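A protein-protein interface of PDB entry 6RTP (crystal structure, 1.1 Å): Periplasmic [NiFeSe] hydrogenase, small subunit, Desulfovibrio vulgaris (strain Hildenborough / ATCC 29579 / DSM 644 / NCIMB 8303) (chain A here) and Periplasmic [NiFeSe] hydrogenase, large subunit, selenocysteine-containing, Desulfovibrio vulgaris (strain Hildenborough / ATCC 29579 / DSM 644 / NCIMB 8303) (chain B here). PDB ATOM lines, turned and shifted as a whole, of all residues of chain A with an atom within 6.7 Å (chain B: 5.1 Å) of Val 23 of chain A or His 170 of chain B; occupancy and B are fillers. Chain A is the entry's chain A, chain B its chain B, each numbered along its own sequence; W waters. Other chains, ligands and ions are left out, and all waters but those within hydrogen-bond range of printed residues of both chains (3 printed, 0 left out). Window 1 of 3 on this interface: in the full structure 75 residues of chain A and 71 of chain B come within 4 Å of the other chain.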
ATOM      1  N   TRP A  12      41.962 -27.068  20.039  1.00  0.00           N
ATOM      2  CA  TRP A  12      40.612 -27.324  19.557  1.00  0.00           C
ATOM      3  C   TRP A  12      40.408 -26.465  18.321  1.00  0.00           C
ATOM      4  O   TRP A  12      40.335 -25.234  18.423  1.00  0.00           O
ATOM      5  CB  TRP A  12      39.610 -26.960  20.647  1.00  0.00           C
ATOM      6  CG  TRP A  12      38.195 -27.347  20.398  1.00  0.00           C
ATOM      7  CD1 TRP A  12      37.367 -26.895  19.410  1.00  0.00           C
ATOM      8  CD2 TRP A  12      37.411 -28.228  21.199  1.00  0.00           C
ATOM      9  NE1 TRP A  12      36.130 -27.461  19.538  1.00  0.00           N
ATOM     10  CE2 TRP A  12      36.127 -28.284  20.629  1.00  0.00           C
ATOM     11  CE3 TRP A  12      37.673 -28.977  22.347  1.00  0.00           C
ATOM     12  CZ2 TRP A  12      35.112 -29.062  21.170  1.00  0.00           C
ATOM     13  CZ3 TRP A  12      36.675 -29.750  22.872  1.00  0.00           C
ATOM     14  CH2 TRP A  12      35.409 -29.789  22.286  1.00  0.00           C
ATOM     15  N   CYS A  18      29.152 -25.985  14.315  1.00  0.00           N
ATOM     16  CA  CYS A  18      28.160 -25.048  14.824  1.00  0.00           C
ATOM     17  C   CYS A  18      28.459 -24.615  16.252  1.00  0.00           C
ATOM     18  O   CYS A  18      27.660 -23.890  16.848  1.00  0.00           O
ATOM     19  CB  CYS A  18      26.749 -25.648  14.732  1.00  0.00           C
ATOM     20  SG  CYS A  18      26.266 -26.786  16.050  1.00  0.00           S
ATOM     21  N   THR A  19      29.587 -25.047  16.811  1.00  0.00           N
ATOM     22  CA  THR A  19      30.001 -24.782  18.187  1.00  0.00           C
ATOM     23  C   THR A  19      29.189 -25.617  19.178  1.00  0.00           C
ATOM     24  O   THR A  19      29.445 -25.554  20.395  1.00  0.00           O
ATOM     25  CB  THR A  19      30.050 -23.274  18.464  1.00  0.00           C
ATOM     26  OG1 THR A  19      30.849 -22.669  17.429  1.00  0.00           O
ATOM     27  CG2 THR A  19      30.698 -22.946  19.805  1.00  0.00           C
ATOM     28  N   GLY A  20      28.290 -26.470  18.694  1.00  0.00           N
ATOM     29  CA  GLY A  20      27.523 -27.304  19.590  1.00  0.00           C
ATOM     30  C   GLY A  20      28.357 -28.320  20.344  1.00  0.00           C
ATOM     31  O   GLY A  20      27.986 -28.738  21.445  1.00  0.00           O
ATOM     32  N   CYS A  21      29.477 -28.726  19.768  1.00  0.00           N
ATOM     33  CA  CYS A  21      30.314 -29.706  20.423  1.00  0.00           C
ATOM     34  C   CYS A  21      31.132 -29.059  21.547  1.00  0.00           C
ATOM     35  O   CYS A  21      31.458 -29.725  22.535  1.00  0.00           O
ATOM     36  CB  CYS A  21      31.134 -30.445  19.346  1.00  0.00           C
ATOM     37  SG  CYS A  21      30.191 -31.548  18.180  1.00  0.00           S
ATOM     38  N   SER A  22      31.424 -27.754  21.445  1.00  0.00           N
ATOM     39  CA  SER A  22      31.978 -27.008  22.564  1.00  0.00           C
ATOM     40  C   SER A  22      30.914 -26.769  23.629  1.00  0.00           C
ATOM     41  O   SER A  22      31.169 -26.936  24.821  1.00  0.00           O
ATOM     42  CB  SER A  22      32.543 -25.676  22.096  1.00  0.00           C
ATOM     43  OG  SER A  22      33.735 -25.832  21.354  1.00  0.00           O
ATOM     44  N   VAL A  23      29.711 -26.363  23.217  1.00  0.00           N
ATOM     45  CA  VAL A  23      28.658 -26.090  24.194  1.00  0.00           C
ATOM     46  C   VAL A  23      28.284 -27.341  24.971  1.00  0.00           C
ATOM     47  O   VAL A  23      28.101 -27.293  26.198  1.00  0.00           O
ATOM     48  CB  VAL A  23      27.451 -25.442  23.501  1.00  0.00           C
ATOM     49  CG1 VAL A  23      26.317 -25.290  24.473  1.00  0.00           C
ATOM     50  CG2 VAL A  23      27.829 -24.079  22.935  1.00  0.00           C
ATOM     51  N   THR A  24      28.171 -28.482  24.288  1.00  0.00           N
ATOM     52  CA  THR A  24      27.822 -29.698  25.005  1.00  0.00           C
ATOM     53  C   THR A  24      28.875 -30.026  26.057  1.00  0.00           C
ATOM     54  O   THR A  24      28.544 -30.465  27.161  1.00  0.00           O
ATOM     55  CB  THR A  24      27.562 -30.841  24.023  1.00  0.00           C
ATOM     56  OG1 THR A  24      26.667 -31.768  24.643  1.00  0.00           O
ATOM     57  CG2 THR A  24      28.840 -31.581  23.600  1.00  0.00           C
ATOM     58  N   LEU A  25      30.149 -29.801  25.742  1.00  0.00           N
ATOM     59  CA  LEU A  25      31.207 -30.052  26.708  1.00  0.00           C
ATOM     60  C   LEU A  25      31.060 -29.148  27.922  1.00  0.00           C
ATOM     61  O   LEU A  25      31.299 -29.586  29.054  1.00  0.00           O
ATOM     62  CB  LEU A  25      32.551 -29.831  26.027  1.00  0.00           C
ATOM     63  CG  LEU A  25      33.774 -29.947  26.917  1.00  0.00           C
ATOM     64  CD1 LEU A  25      33.848 -31.315  27.575  1.00  0.00           C
ATOM     65  CD2 LEU A  25      35.024 -29.681  26.121  1.00  0.00           C
ATOM     66  N   LEU A  26      30.680 -27.883  27.711  1.00  0.00           N
ATOM     67  CA  LEU A  26      30.435 -26.974  28.827  1.00  0.00           C
ATOM     68  C   LEU A  26      29.364 -27.505  29.769  1.00  0.00           C
ATOM     69  O   LEU A  26      29.329 -27.102  30.938  1.00  0.00           O
ATOM     70  CB  LEU A  26      29.991 -25.594  28.330  1.00  0.00           C
ATOM     71  CG  LEU A  26      30.949 -24.830  27.415  1.00  0.00           C
ATOM     72  CD1 LEU A  26      30.353 -23.475  27.021  1.00  0.00           C
ATOM     73  CD2 LEU A  26      32.312 -24.683  28.035  1.00  0.00           C
ATOM     74  N   ASN A  27      28.494 -28.406  29.298  1.00  0.00           N
ATOM     75  CA  ASN A  27      27.454 -28.989  30.136  1.00  0.00           C
ATOM     76  C   ASN A  27      27.898 -30.201  30.951  1.00  0.00           C
ATOM     77  O   ASN A  27      27.065 -30.800  31.640  1.00  0.00           O
ATOM     78  CB  ASN A  27      26.237 -29.352  29.291  1.00  0.00           C
ATOM     79  CG  ASN A  27      25.498 -28.135  28.786  1.00  0.00           C
ATOM     80  OD1 ASN A  27      25.587 -27.039  29.348  1.00  0.00           O
ATOM     81  ND2 ASN A  27      24.724 -28.329  27.721  1.00  0.00           N
ATOM     82  N   SER A  28      29.178 -30.577  30.927  1.00  0.00           N
ATOM     83  CA  SER A  28      29.619 -31.727  31.711  1.00  0.00           C
ATOM     84  C   SER A  28      29.285 -31.566  33.195  1.00  0.00           C
ATOM     85  O   SER A  28      29.558 -30.532  33.803  1.00  0.00           O
ATOM     86  CB  SER A  28      31.124 -31.897  31.534  1.00  0.00           C
ATOM     87  OG  SER A  28      31.556 -33.078  32.186  1.00  0.00           O
ATOM     88  N   THR A  48      36.666 -20.113  20.787  1.00  0.00           N
ATOM     89  CA  THR A  48      35.454 -19.624  21.436  1.00  0.00           C
ATOM     90  C   THR A  48      35.731 -19.081  22.824  1.00  0.00           C
ATOM     91  O   THR A  48      35.008 -18.187  23.279  1.00  0.00           O
ATOM     92  CB  THR A  48      34.411 -20.746  21.524  1.00  0.00           C
ATOM     93  OG1 THR A  48      34.324 -21.454  20.281  1.00  0.00           O
ATOM     94  CG2 THR A  48      33.036 -20.192  21.904  1.00  0.00           C
ATOM     95  N   GLU A  77      36.349 -30.118  15.546  1.00  0.00           N
ATOM     96  CA  GLU A  77      34.894 -29.924  15.621  1.00  0.00           C
ATOM     97  C   GLU A  77      34.448 -29.347  14.278  1.00  0.00           C
ATOM     98  O   GLU A  77      34.893 -28.257  13.911  1.00  0.00           O
ATOM     99  CB  GLU A  77      34.550 -28.948  16.771  1.00  0.00           C
ATOM    100  CG  GLU A  77      33.092 -28.366  16.807  1.00  0.00           C
ATOM    101  CD  GLU A  77      32.783 -27.455  18.024  1.00  0.00           C
ATOM    102  OE1 GLU A  77      33.706 -26.857  18.628  1.00  0.00           O
ATOM    103  OE2 GLU A  77      31.576 -27.311  18.371  1.00  0.00           O
ATOM    104  N   PRO A 160      24.681 -32.826  19.070  1.00  0.00           N
ATOM    105  CA  PRO A 160      26.060 -32.986  19.514  1.00  0.00           C
ATOM    106  C   PRO A 160      26.263 -34.296  20.280  1.00  0.00           C
ATOM    107  O   PRO A 160      25.307 -34.955  20.671  1.00  0.00           O
ATOM    108  CB  PRO A 160      26.227 -31.818  20.486  1.00  0.00           C
ATOM    109  CG  PRO A 160      24.905 -31.739  21.151  1.00  0.00           C
ATOM    110  CD  PRO A 160      23.893 -32.094  20.080  1.00  0.00           C
ATOM    111  N   PRO A 163      28.316 -34.643  26.690  1.00  0.00           N
ATOM    112  CA  PRO A 163      29.609 -34.297  27.310  1.00  0.00           C
ATOM    113  C   PRO A 163      30.340 -35.503  27.855  1.00  0.00           C
ATOM    114  O   PRO A 163      31.580 -35.555  27.792  1.00  0.00           O
ATOM    115  CB  PRO A 163      29.240 -33.301  28.422  1.00  0.00           C
ATOM    116  CG  PRO A 163      27.781 -33.503  28.657  1.00  0.00           C
ATOM    117  CD  PRO A 163      27.208 -33.875  27.283  1.00  0.00           C
ATOM    118  N   ASN A 253      21.587 -33.737  29.815  1.00  0.00           N
ATOM    119  CA  ASN A 253      21.487 -32.502  30.595  1.00  0.00           C
ATOM    120  C   ASN A 253      21.181 -32.798  32.061  1.00  0.00           C
ATOM    121  O   ASN A 253      20.169 -32.372  32.624  1.00  0.00           O
ATOM    122  CB  ASN A 253      20.480 -31.542  29.966  1.00  0.00           C
ATOM    123  CG  ASN A 253      20.867 -31.160  28.558  1.00  0.00           C
ATOM    124  OD1 ASN A 253      20.420 -31.770  27.573  1.00  0.00           O
ATOM    125  ND2 ASN A 253      21.751 -30.183  28.451  1.00  0.00           N
ATOM    126  N   VAL A 256      17.845 -35.124  32.966  1.00  0.00           N
ATOM    127  CA  VAL A 256      16.476 -34.603  33.070  1.00  0.00           C
ATOM    128  C   VAL A 256      15.564 -35.079  31.947  1.00  0.00           C
ATOM    129  O   VAL A 256      14.337 -34.960  32.069  1.00  0.00           O
ATOM    130  CB  VAL A 256      16.412 -33.066  33.173  1.00  0.00           C
ATOM    131  CG1 VAL A 256      17.166 -32.579  34.386  1.00  0.00           C
ATOM    132  CG2 VAL A 256      16.883 -32.370  31.890  1.00  0.00           C
ATOM    133  N   GLY B  73      25.003 -24.052  17.549  1.00  0.00           N
ATOM    134  CA  GLY B  73      24.799 -24.758  18.790  1.00  0.00           C
ATOM    135  C   GLY B  73      24.688 -23.908  20.034  1.00  0.00           C
ATOM    136  O   GLY B  73      24.427 -24.440  21.116  1.00  0.00           O
ATOM    137  N   VAL B  74      24.893 -22.608  19.876  1.00  0.00           N
ATOM    138  CA  VAL B  74      24.684 -21.658  20.963  1.00  0.00           C
ATOM    139  C   VAL B  74      23.231 -21.194  21.007  1.00  0.00           C
ATOM    140  O   VAL B  74      22.644 -21.097  22.087  1.00  0.00           O
ATOM    141  CB  VAL B  74      25.654 -20.466  20.853  1.00  0.00           C
ATOM    142  CG1 VAL B  74      25.404 -19.462  21.962  1.00  0.00           C
ATOM    143  CG2 VAL B  74      27.104 -20.936  20.867  1.00  0.00           C
ATOM    144  N   ASN B 110      16.881 -20.647  27.203  1.00  0.00           N
ATOM    145  CA  ASN B 110      18.137 -20.448  26.498  1.00  0.00           C
ATOM    146  C   ASN B 110      18.538 -18.986  26.381  1.00  0.00           C
ATOM    147  O   ASN B 110      19.727 -18.721  26.205  1.00  0.00           O
ATOM    148  CB  ASN B 110      18.204 -21.130  25.132  1.00  0.00           C
ATOM    149  CG  ASN B 110      19.641 -21.352  24.713  1.00  0.00           C
ATOM    150  OD1 ASN B 110      20.421 -21.908  25.480  1.00  0.00           O
ATOM    151  ND2 ASN B 110      20.005 -20.885  23.543  1.00  0.00           N
ATOM    152  N   GLN B 113      20.640 -18.791  29.372  1.00  0.00           N
ATOM    153  CA  GLN B 113      21.921 -19.453  29.130  1.00  0.00           C
ATOM    154  C   GLN B 113      22.831 -18.590  28.278  1.00  0.00           C
ATOM    155  O   GLN B 113      24.027 -18.462  28.563  1.00  0.00           O
ATOM    156  CB  GLN B 113      21.703 -20.786  28.408  1.00  0.00           C
ATOM    157  CG  GLN B 113      23.016 -21.596  28.203  1.00  0.00           C
ATOM    158  CD  GLN B 113      23.817 -21.333  26.921  1.00  0.00           C
ATOM    159  OE1 GLN B 113      25.033 -21.529  26.922  1.00  0.00           O
ATOM    160  NE2 GLN B 113      23.162 -20.955  25.825  1.00  0.00           N
ATOM    161  N   ARG B 166      24.948 -21.525  33.739  1.00  0.00           N
ATOM    162  CA  ARG B 166      24.546 -21.722  32.346  1.00  0.00           C
ATOM    163  C   ARG B 166      24.210 -23.179  32.073  1.00  0.00           C
ATOM    164  O   ARG B 166      23.323 -23.471  31.262  1.00  0.00           O
ATOM    165  CB  ARG B 166      25.583 -21.178  31.350  1.00  0.00           C
ATOM    166  CG  ARG B 166      26.958 -21.832  31.372  1.00  0.00           C
ATOM    167  CD  ARG B 166      27.617 -21.878  29.976  1.00  0.00           C
ATOM    168  NE  ARG B 166      26.756 -22.531  28.989  1.00  0.00           N
ATOM    169  CZ  ARG B 166      26.441 -23.826  28.980  1.00  0.00           C
ATOM    170  NH1 ARG B 166      26.957 -24.659  29.861  1.00  0.00           N
ATOM    171  NH2 ARG B 166      25.600 -24.295  28.069  1.00  0.00           N
ATOM    172  N   ARG B 167      24.897 -24.100  32.745  1.00  0.00           N
ATOM    173  CA  ARG B 167      24.569 -25.513  32.613  1.00  0.00           C
ATOM    174  C   ARG B 167      23.165 -25.793  33.131  1.00  0.00           C
ATOM    175  O   ARG B 167      22.397 -26.537  32.512  1.00  0.00           O
ATOM    176  CB  ARG B 167      25.620 -26.351  33.339  1.00  0.00           C
ATOM    177  CG  ARG B 167      25.368 -27.857  33.223  1.00  0.00           C
ATOM    178  CD  ARG B 167      26.339 -28.708  34.027  1.00  0.00           C
ATOM    179  NE  ARG B 167      26.351 -28.356  35.443  1.00  0.00           N
ATOM    180  CZ  ARG B 167      25.400 -28.652  36.319  1.00  0.00           C
ATOM    181  NH1 ARG B 167      24.316 -29.314  35.951  1.00  0.00           N
ATOM    182  NH2 ARG B 167      25.540 -28.278  37.590  1.00  0.00           N
ATOM    183  N   ILE B 168      22.823 -25.220  34.283  1.00  0.00           N
ATOM    184  CA  ILE B 168      21.483 -25.356  34.843  1.00  0.00           C
ATOM    185  C   ILE B 168      20.439 -24.789  33.888  1.00  0.00           C
ATOM    186  O   ILE B 168      19.342 -25.336  33.753  1.00  0.00           O
ATOM    187  CB  ILE B 168      21.440 -24.678  36.229  1.00  0.00           C
ATOM    188  CG1 ILE B 168      22.256 -25.487  37.238  1.00  0.00           C
ATOM    189  CG2 ILE B 168      19.999 -24.503  36.717  1.00  0.00           C
ATOM    190  CD1 ILE B 168      22.569 -24.759  38.554  1.00  0.00           C
ATOM    191  N   CYS B 169      20.762 -23.693  33.197  1.00  0.00           N
ATOM    192  CA  CYS B 169      19.836 -23.172  32.198  1.00  0.00           C
ATOM    193  C   CYS B 169      19.557 -24.208  31.113  1.00  0.00           C
ATOM    194  O   CYS B 169      18.422 -24.340  30.646  1.00  0.00           O
ATOM    195  CB  CYS B 169      20.366 -21.891  31.559  1.00  0.00           C
ATOM    196  SG  CYS B 169      20.435 -20.434  32.651  1.00  0.00           S
ATOM    197  N   HIS B 170      20.588 -24.939  30.683  1.00  0.00           N
ATOM    198  CA  HIS B 170      20.363 -25.986  29.693  1.00  0.00           C
ATOM    199  C   HIS B 170      19.565 -27.158  30.260  1.00  0.00           C
ATOM    200  O   HIS B 170      18.808 -27.795  29.519  1.00  0.00           O
ATOM    201  CB  HIS B 170      21.675 -26.417  29.035  1.00  0.00           C
ATOM    202  CG  HIS B 170      21.994 -25.611  27.828  1.00  0.00           C
ATOM    203  ND1 HIS B 170      23.058 -25.898  26.995  1.00  0.00           N
ATOM    204  CD2 HIS B 170      21.386 -24.511  27.322  1.00  0.00           C
ATOM    205  CE1 HIS B 170      23.059 -25.024  26.005  1.00  0.00           C
ATOM    206  NE2 HIS B 170      22.065 -24.168  26.186  1.00  0.00           N
ATOM    207  N   GLU B 171      19.686 -27.451  31.556  1.00  0.00           N
ATOM    208  CA  GLU B 171      18.764 -28.405  32.152  1.00  0.00           C
ATOM    209  C   GLU B 171      17.327 -27.915  32.039  1.00  0.00           C
ATOM    210  O   GLU B 171      16.416 -28.700  31.760  1.00  0.00           O
ATOM    211  CB  GLU B 171      19.120 -28.683  33.614  1.00  0.00           C
ATOM    212  CG  GLU B 171      20.477 -29.321  33.780  1.00  0.00           C
ATOM    213  CD  GLU B 171      20.769 -29.799  35.184  1.00  0.00           C
ATOM    214  OE1 GLU B 171      20.034 -29.432  36.118  1.00  0.00           O
ATOM    215  OE2 GLU B 171      21.749 -30.562  35.343  1.00  0.00           O
ATOM    216  N   MET B 172      17.100 -26.625  32.291  1.00  0.00           N
ATOM    217  CA  MET B 172      15.759 -26.070  32.123  1.00  0.00           C
ATOM    218  C   MET B 172      15.260 -26.249  30.697  1.00  0.00           C
ATOM    219  O   MET B 172      14.096 -26.613  30.493  1.00  0.00           O
ATOM    220  CB  MET B 172      15.742 -24.596  32.517  1.00  0.00           C
ATOM    221  CG  MET B 172      15.970 -24.354  34.013  1.00  0.00           C
ATOM    222  SD  MET B 172      16.387 -22.639  34.395  1.00  0.00           S
ATOM    223  CE  MET B 172      14.950 -21.805  33.707  1.00  0.00           C
ATOM    224  N   VAL B 173      16.109 -25.967  29.701  1.00  0.00           N
ATOM    225  CA  VAL B 173      15.706 -26.157  28.304  1.00  0.00           C
ATOM    226  C   VAL B 173      15.325 -27.609  28.055  1.00  0.00           C
ATOM    227  O   VAL B 173      14.321 -27.905  27.391  1.00  0.00           O
ATOM    228  CB  VAL B 173      16.835 -25.742  27.342  1.00  0.00           C
ATOM    229  CG1 VAL B 173      16.461 -26.059  25.901  1.00  0.00           C
ATOM    230  CG2 VAL B 173      17.191 -24.269  27.466  1.00  0.00           C
ATOM    231  N   ALA B 174      16.147 -28.537  28.556  1.00  0.00           N
ATOM    232  CA  ALA B 174      15.950 -29.948  28.263  1.00  0.00           C
ATOM    233  C   ALA B 174      14.731 -30.543  28.960  1.00  0.00           C
ATOM    234  O   ALA B 174      14.200 -31.558  28.495  1.00  0.00           O
ATOM    235  CB  ALA B 174      17.210 -30.718  28.657  1.00  0.00           C
ATOM    236  N   LEU B 175      14.273 -29.962  30.070  1.00  0.00           N
ATOM    237  CA  LEU B 175      13.130 -30.534  30.779  1.00  0.00           C
ATOM    238  C   LEU B 175      11.944 -30.764  29.851  1.00  0.00           C
ATOM    239  O   LEU B 175      11.343 -31.837  29.860  1.00  0.00           O
ATOM    240  CB  LEU B 175      12.761 -29.669  31.982  1.00  0.00           C
ATOM    241  CG  LEU B 175      13.578 -29.968  33.250  1.00  0.00           C
ATOM    242  CD1 LEU B 175      13.407 -28.830  34.257  1.00  0.00           C
ATOM    243  CD2 LEU B 175      13.175 -31.285  33.882  1.00  0.00           C
ATOM    244  N   MET B 180      19.842 -30.477  25.036  1.00  0.00           N
ATOM    245  CA  MET B 180      20.366 -29.203  24.568  1.00  0.00           C
ATOM    246  C   MET B 180      21.879 -29.302  24.590  1.00  0.00           C
ATOM    247  O   MET B 180      22.432 -29.793  25.586  1.00  0.00           O
ATOM    248  CB  MET B 180      19.881 -28.066  25.471  1.00  0.00           C
ATOM    249  CG  MET B 180      20.156 -26.705  24.979  1.00  0.00           C
ATOM    250  SD  MET B 180      19.304 -26.264  23.443  1.00  0.00           S
ATOM    251  CE  MET B 180      19.575 -24.507  23.511  1.00  0.00           C
ATOM    252  N   PRO B 181      22.591 -28.836  23.552  1.00  0.00           N
ATOM    253  CA  PRO B 181      22.115 -28.294  22.281  1.00  0.00           C
ATOM    254  C   PRO B 181      21.211 -29.237  21.502  1.00  0.00           C
ATOM    255  O   PRO B 181      21.287 -30.454  21.629  1.00  0.00           O
ATOM    256  CB  PRO B 181      23.409 -28.059  21.485  1.00  0.00           C
ATOM    257  CG  PRO B 181      24.465 -27.850  22.513  1.00  0.00           C
ATOM    258  CD  PRO B 181      24.059 -28.773  23.656  1.00  0.00           C
HETATM  259  O   HOH W   1      29.211 -24.365  31.592  1.00  0.00           O
HETATM  260  O   HOH W   2      24.686 -31.153  26.519  1.00  0.00           O
HETATM  261  O   HOH W   3      22.847 -29.049  30.945  1.00  0.00           O
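The side-chain amide oxygen (OD1) of Asn 253 of chain A is in hydrogen-bond range of the backbone NH (N) of Met 180 of chain B, at 2.9 Å.
The side-chain amide oxygen (OD1) of Asn 27 of chain A lies within hydrogen-bond range of the guanidinium group (NH1) of Arg 166 of chain B (2.8 Å).
O of Met 180 of chain B lies within hydrogen-bond range of ND2 of Asn 27 of chain A.
The side-chain amide nitrogen of Asn 27 of chain A sits at hydrogen-bond distance from a ring nitrogen (ND1) of His 170 of chain B (3.0 Å).
The backbone NH (N) of Gly 73 of chain B sits at hydrogen-bond distance from the backbone carbonyl oxygen (O) of Cys 18 of chain A.
Among the printed residues, pairs that only touch across the chains: Gly 20 of chain A with Gly 73 of chain B, Gly 20 of chain A with Pro 181 of chain B, Val 23 of chain A with Gly 73 of chain B, Val 23 of chain A with Val 74 of chain B, Val 23 of chain A with Arg 166 of chain B, Val 23 of chain A with His 170 of chain B, Val 23 of chain A with Pro 181 of chain B, Leu 26 of chain A with Arg 166 of chain B, Asn 27 of chain A with Arg 167 of chain B, Ser 28 of chain A with Arg 167 of chain B, Pro 160 of chain A with Pro 181 of chain B, Asn 253 of chain A with His 170 of chain B, Asn 253 of chain A with Glu 171 of chain B, Asn 253 of chain A with Ala 174 of chain B, Val 256 of chain A with Glu 171 of chain B, Val 256 of chain A with Ala 174 of chain B and Val 256 of chain A with Leu 175 of chain B.
Printed residues of chain A that touch a printed residue of chain B: Cys 18, Gly 20, Val 23, Leu 26, Asn 27, Ser 28, Pro 160, Asn 253 and Val 256.
Printed residues of chain B that touch a printed residue of chain A: Gly 73, Val 74, Arg 166, Arg 167, His 170, Glu 171, Ala 174, Leu 175, Met 180 and Pro 181.
Hydrophobic or aromatic side chains of chain B within 4 Å of the printed part of chain A: Val 74, His 170, Ala 174, Leu 175 and Pro 181.
Among the printed residues, no Asp or Glu carboxylate lies within 4 Å of a Lys or Arg side-chain nitrogen of the other chain.
The side-chain carboxylate (OE2) of Glu 171 of chain B lies within salt-bridge range of the guanidinium group (NH1) of Arg 167 of chain B (2.9 Å).
ND1 of His 170 of chain B is in hydrogen-bond range of NH2 of Arg 166 of chain B (3.2 Å).
The side-chain amide nitrogen (NE2) of Gln 113 of chain B sits close to a ring nitrogen (NE2) of His 170 of chain B (3.4 Å).
OE1 of Gln 113 of chain B sits at hydrogen-bond distance from NE of Arg 166 of chain B (2.9 Å).
The backbone carbonyl oxygen of Val 74 of chain B is in hydrogen-bond range of the side-chain amide nitrogen of Asn 110 of chain B (3.0 Å).
The side-chain amide oxygen (OD1) of Asn 110 of chain B sits at hydrogen-bond distance from a ring nitrogen (NE2) of His 170 of chain B (2.9 Å).
Water W2 lies within hydrogen-bond range of the backbone carbonyl oxygen of Met 180 of chain B (2.8 Å), the side-chain hydroxyl of Thr 24 of chain A (2.8 Å) and the side-chain amide nitrogen of Asn 27 of chain A (3.1 Å).
Water W1 bridges O of Leu 26 of chain A and NH1 of Arg 166 of chain B.
Water W3 bridges the side-chain amide nitrogen of Asn 253 of chain A (3.0 Å) and the backbone carbonyl oxygen of Arg 167 of chain B (3.0 Å).
Thr 19 of chain A touches none of the printed residues of chain B.
Of chain B, only Gly 73, Val 74, Arg 166, His 170 and Pro 181 come within 4 Å of Val 23 of chain A.
Of the printed residues of chain B, Leu 26 of chain A touches Arg 166.
Thr 48 of chain A touches none of the printed residues of chain B.
Printed residues of chain B within 4 Å of Pro 160 of chain A: Pro 181 (3.4 Å).
His 170 of chain B touches just these residues of chain A: Val 23 (3.6 Å), Asn 27 (3.0 Å) and Asn 253 (3.8 Å).
Of the printed residues of chain A, Leu 175 of chain B touches Val 256.
The nearest residue of chain B that does not touch Val 23 of chain A is Gln 113 of chain B (4.7 Å).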
